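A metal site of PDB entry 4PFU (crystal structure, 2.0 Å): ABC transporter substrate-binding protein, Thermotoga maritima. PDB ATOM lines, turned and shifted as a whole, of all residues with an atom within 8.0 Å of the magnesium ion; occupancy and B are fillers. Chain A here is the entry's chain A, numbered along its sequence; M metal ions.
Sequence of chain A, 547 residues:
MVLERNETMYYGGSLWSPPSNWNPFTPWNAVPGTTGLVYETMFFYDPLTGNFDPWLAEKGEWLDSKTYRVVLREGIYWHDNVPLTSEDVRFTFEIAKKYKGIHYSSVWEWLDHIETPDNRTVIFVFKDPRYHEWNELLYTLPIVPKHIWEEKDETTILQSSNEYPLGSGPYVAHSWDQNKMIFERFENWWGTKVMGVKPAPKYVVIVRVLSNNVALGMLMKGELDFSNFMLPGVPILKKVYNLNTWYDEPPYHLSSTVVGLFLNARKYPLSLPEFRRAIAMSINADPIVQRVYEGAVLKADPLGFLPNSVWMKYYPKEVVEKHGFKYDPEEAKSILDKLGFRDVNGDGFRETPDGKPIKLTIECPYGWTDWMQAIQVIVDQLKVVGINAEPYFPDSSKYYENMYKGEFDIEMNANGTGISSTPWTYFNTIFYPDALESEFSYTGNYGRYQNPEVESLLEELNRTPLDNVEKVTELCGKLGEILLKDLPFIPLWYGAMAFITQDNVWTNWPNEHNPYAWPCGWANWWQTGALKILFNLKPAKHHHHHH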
ATOM      1  N   ARG A 342      15.577 -12.196  28.190  1.00  0.00           N
ATOM      2  CA  ARG A 342      14.857 -10.933  28.028  1.00  0.00           C
ATOM      3  C   ARG A 342      15.667  -9.907  27.250  1.00  0.00           C
ATOM      4  O   ARG A 342      16.896  -9.970  27.167  1.00  0.00           O
ATOM      5  CB  ARG A 342      14.456 -10.376  29.399  1.00  0.00           C
ATOM      6  CG  ARG A 342      13.261 -11.101  29.972  1.00  0.00           C
ATOM      7  CD  ARG A 342      13.036 -10.826  31.441  1.00  0.00           C
ATOM      8  NE  ARG A 342      11.701 -11.273  31.831  1.00  0.00           N
ATOM      9  CZ  ARG A 342      11.349 -11.597  33.074  1.00  0.00           C
ATOM     10  NH1 ARG A 342      12.235 -11.535  34.058  1.00  0.00           N
ATOM     11  NH2 ARG A 342      10.100 -11.992  33.330  1.00  0.00           N
ATOM     12  N   ASP A 343      14.957  -8.937  26.681  1.00  0.00           N
ATOM     13  CA  ASP A 343      15.561  -7.880  25.903  1.00  0.00           C
ATOM     14  C   ASP A 343      16.066  -6.755  26.810  1.00  0.00           C
ATOM     15  O   ASP A 343      15.276  -5.980  27.350  1.00  0.00           O
ATOM     16  CB  ASP A 343      14.536  -7.349  24.891  1.00  0.00           C
ATOM     17  CG  ASP A 343      15.061  -6.199  24.068  1.00  0.00           C
ATOM     18  OD1 ASP A 343      16.288  -5.965  24.073  1.00  0.00           O
ATOM     19  OD2 ASP A 343      14.239  -5.543  23.396  1.00  0.00           O
ATOM     20  N   VAL A 344      17.386  -6.661  26.971  1.00  0.00           N
ATOM     21  CA  VAL A 344      17.960  -5.652  27.864  1.00  0.00           C
ATOM     22  C   VAL A 344      18.581  -4.477  27.125  1.00  0.00           C
ATOM     23  O   VAL A 344      18.939  -3.481  27.751  1.00  0.00           O
ATOM     24  CB  VAL A 344      19.035  -6.270  28.792  1.00  0.00           C
ATOM     25  CG1 VAL A 344      18.427  -7.365  29.659  1.00  0.00           C
ATOM     26  CG2 VAL A 344      20.203  -6.804  27.992  1.00  0.00           C
ATOM     27  N   ASN A 345      18.714  -4.565  25.810  1.00  0.00           N
ATOM     28  CA  ASN A 345      19.278  -3.449  25.035  1.00  0.00           C
ATOM     29  C   ASN A 345      18.236  -2.768  24.142  1.00  0.00           C
ATOM     30  O   ASN A 345      18.544  -1.818  23.433  1.00  0.00           O
ATOM     31  CB  ASN A 345      20.456  -3.926  24.183  1.00  0.00           C
ATOM     32  CG  ASN A 345      20.087  -5.036  23.212  1.00  0.00           C
ATOM     33  OD1 ASN A 345      18.922  -5.192  22.826  1.00  0.00           O
ATOM     34  ND2 ASN A 345      21.070  -5.818  22.809  1.00  0.00           N
ATOM     35  N   GLY A 346      17.013  -3.286  24.155  1.00  0.00           N
ATOM     36  CA  GLY A 346      15.903  -2.654  23.461  1.00  0.00           C
ATOM     37  C   GLY A 346      15.832  -2.846  21.964  1.00  0.00           C
ATOM     38  O   GLY A 346      15.150  -2.087  21.278  1.00  0.00           O
ATOM     39  N   ASP A 347      16.517  -3.846  21.421  1.00  0.00           N
ATOM     40  CA  ASP A 347      16.475  -4.052  19.967  1.00  0.00           C
ATOM     41  C   ASP A 347      15.409  -5.086  19.589  1.00  0.00           C
ATOM     42  O   ASP A 347      15.345  -5.529  18.440  1.00  0.00           O
ATOM     43  CB  ASP A 347      17.841  -4.476  19.426  1.00  0.00           C
ATOM     44  CG  ASP A 347      18.263  -5.856  19.898  1.00  0.00           C
ATOM     45  OD1 ASP A 347      17.554  -6.462  20.723  1.00  0.00           O
ATOM     46  OD2 ASP A 347      19.324  -6.339  19.430  1.00  0.00           O
ATOM     47  N   GLY A 348      14.578  -5.463  20.548  1.00  0.00           N
ATOM     48  CA  GLY A 348      13.498  -6.401  20.291  1.00  0.00           C
ATOM     49  C   GLY A 348      13.926  -7.848  20.395  1.00  0.00           C
ATOM     50  O   GLY A 348      13.091  -8.742  20.409  1.00  0.00           O
ATOM     51  N   PHE A 349      15.235  -8.079  20.479  1.00  0.00           N
ATOM     52  CA  PHE A 349      15.763  -9.438  20.602  1.00  0.00           C
ATOM     53  C   PHE A 349      16.095  -9.780  22.059  1.00  0.00           C
ATOM     54  O   PHE A 349      16.586  -8.939  22.814  1.00  0.00           O
ATOM     55  CB  PHE A 349      17.007  -9.601  19.723  1.00  0.00           C
ATOM     56  CG  PHE A 349      16.700  -9.606  18.245  1.00  0.00           C
ATOM     57  CD1 PHE A 349      15.672 -10.394  17.740  1.00  0.00           C
ATOM     58  CD2 PHE A 349      17.431  -8.817  17.365  1.00  0.00           C
ATOM     59  CE1 PHE A 349      15.390 -10.392  16.385  1.00  0.00           C
ATOM     60  CE2 PHE A 349      17.150  -8.814  16.010  1.00  0.00           C
ATOM     61  CZ  PHE A 349      16.121  -9.603  15.519  1.00  0.00           C
ATOM     62  N   ARG A 350      15.812 -11.010  22.447  1.00  0.00           N
ATOM     63  CA  ARG A 350      16.094 -11.429  23.810  1.00  0.00           C
ATOM     64  C   ARG A 350      17.560 -11.831  23.951  1.00  0.00           C
ATOM     65  O   ARG A 350      18.110 -12.541  23.100  1.00  0.00           O
ATOM     66  CB  ARG A 350      15.184 -12.588  24.217  1.00  0.00           C
ATOM     67  CG  ARG A 350      13.724 -12.229  24.201  1.00  0.00           C
ATOM     68  CD  ARG A 350      12.876 -13.481  24.184  1.00  0.00           C
ATOM     69  NE  ARG A 350      11.447 -13.176  24.193  1.00  0.00           N
ATOM     70  CZ  ARG A 350      10.759 -12.877  25.288  1.00  0.00           C
ATOM     71  NH1 ARG A 350      11.369 -12.850  26.469  1.00  0.00           N
ATOM     72  NH2 ARG A 350       9.462 -12.619  25.207  1.00  0.00           N
ATOM     73  N   GLU A 351      18.187 -11.349  25.015  1.00  0.00           N
ATOM     74  CA  GLU A 351      19.555 -11.731  25.359  1.00  0.00           C
ATOM     75  C   GLU A 351      19.521 -12.910  26.323  1.00  0.00           C
ATOM     76  O   GLU A 351      18.459 -13.307  26.795  1.00  0.00           O
ATOM     77  CB  GLU A 351      20.314 -10.548  25.977  1.00  0.00           C
ATOM     78  CG  GLU A 351      20.843  -9.546  24.963  1.00  0.00           C
ATOM     79  CD  GLU A 351      19.761  -8.657  24.363  1.00  0.00           C
ATOM     80  OE1 GLU A 351      19.725  -8.520  23.122  1.00  0.00           O
ATOM     81  OE2 GLU A 351      18.970  -8.079  25.135  1.00  0.00           O
ATOM     82  N   THR A 352      20.692 -13.479  26.607  1.00  0.00           N
ATOM     83  CA  THR A 352      20.796 -14.530  27.610  1.00  0.00           C
ATOM     84  C   THR A 352      20.531 -13.947  28.989  1.00  0.00           C
ATOM     85  O   THR A 352      20.558 -12.730  29.164  1.00  0.00           O
ATOM     86  CB  THR A 352      22.188 -15.176  27.599  1.00  0.00           C
ATOM     87  OG1 THR A 352      23.153 -14.221  28.044  1.00  0.00           O
ATOM     88  CG2 THR A 352      22.540 -15.683  26.202  1.00  0.00           C
ATOM     89  N   GLY A 355      22.877 -11.406  29.916  1.00  0.00           N
ATOM     90  CA  GLY A 355      22.925 -10.215  29.067  1.00  0.00           C
ATOM     91  C   GLY A 355      23.748 -10.355  27.800  1.00  0.00           C
ATOM     92  O   GLY A 355      24.106  -9.355  27.177  1.00  0.00           O
ATOM     93  N   LYS A 356      24.043 -11.590  27.419  1.00  0.00           N
ATOM     94  CA  LYS A 356      24.794 -11.863  26.194  1.00  0.00           C
ATOM     95  C   LYS A 356      23.847 -11.879  24.998  1.00  0.00           C
ATOM     96  O   LYS A 356      22.748 -12.445  25.070  1.00  0.00           O
ATOM     97  CB  LYS A 356      25.536 -13.201  26.308  1.00  0.00           C
ATOM     98  CG  LYS A 356      26.550 -13.508  25.207  1.00  0.00           C
ATOM     99  CD  LYS A 356      26.990 -14.983  25.217  1.00  0.00           C
ATOM    100  CE  LYS A 356      25.780 -15.917  25.139  1.00  0.00           C
ATOM    101  NZ  LYS A 356      25.988 -17.223  25.798  1.00  0.00           N
ATOM    102  N   PRO A 357      24.266 -11.261  23.884  1.00  0.00           N
ATOM    103  CA  PRO A 357      23.398 -11.296  22.704  1.00  0.00           C
ATOM    104  C   PRO A 357      23.244 -12.718  22.165  1.00  0.00           C
ATOM    105  O   PRO A 357      24.089 -13.581  22.423  1.00  0.00           O
ATOM    106  CB  PRO A 357      24.123 -10.393  21.684  1.00  0.00           C
ATOM    107  CG  PRO A 357      25.508 -10.258  22.186  1.00  0.00           C
ATOM    108  CD  PRO A 357      25.463 -10.417  23.683  1.00  0.00           C
ATOM    109  N   ILE A 358      22.143 -12.955  21.462  1.00  0.00           N
ATOM    110  CA  ILE A 358      21.827 -14.256  20.883  1.00  0.00           C
ATOM    111  C   ILE A 358      21.523 -14.086  19.405  1.00  0.00           C
ATOM    112  O   ILE A 358      20.601 -13.370  19.018  1.00  0.00           O
ATOM    113  CB  ILE A 358      20.616 -14.902  21.575  1.00  0.00           C
ATOM    114  CG1 ILE A 358      20.884 -15.096  23.063  1.00  0.00           C
ATOM    115  CG2 ILE A 358      20.251 -16.222  20.907  1.00  0.00           C
ATOM    116  CD1 ILE A 358      19.696 -15.633  23.808  1.00  0.00           C
ATOM    117  N   GLY A 386      11.250 -12.390  19.512  1.00  0.00           N
ATOM    118  CA  GLY A 386      12.514 -11.847  19.993  1.00  0.00           C
ATOM    119  C   GLY A 386      13.680 -12.824  19.880  1.00  0.00           C
ATOM    120  O   GLY A 386      14.613 -12.764  20.681  1.00  0.00           O
HETATM  121 MG    MG M   1      18.042  -7.115  22.879  1.00  0.00          MG
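Five residues have an atom within 4 Å of the magnesium ion: Asp 343, Asn 345, Asp 347, Phe 349 and Glu 351. Along chain A the residues within 4 Å of the magnesium ion span positions 343 to 351. The nearest printed residue that does not touch the magnesium ion is Gly 346 (4.2 Å).
OD1 of Asn 345 is bound to the magnesium ion (2.1 Å). OE1 of Glu 351 is bound to the magnesium ion (2.2 Å). OD1 of Asp 347 is bound to the magnesium ion (2.3 Å). O of Phe 349 is bound to the magnesium ion (2.3 Å). OD1 of Asp 343 binds the magnesium ion, 2.4 Å away. Slightly farther from the magnesium ion lies the side-chain carboxylate (OE2) of Glu 351 (2.6 Å).
The backbone carbonyl oxygen (O) of Arg 342 sits at hydrogen-bond distance from the backbone NH (N) of Glu 351 (2.9 Å). The side-chain carboxylate (OD2) of Asp 343 lies within hydrogen-bond range of the backbone NH (N) of Gly 348 (2.9 Å). The side-chain carboxylate of Glu 351 lies within hydrogen-bond range of the backbone NH of Val 344. The side-chain carboxylate of Asp 343 sits close to the backbone NH of Gly 346 (2.8 Å).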
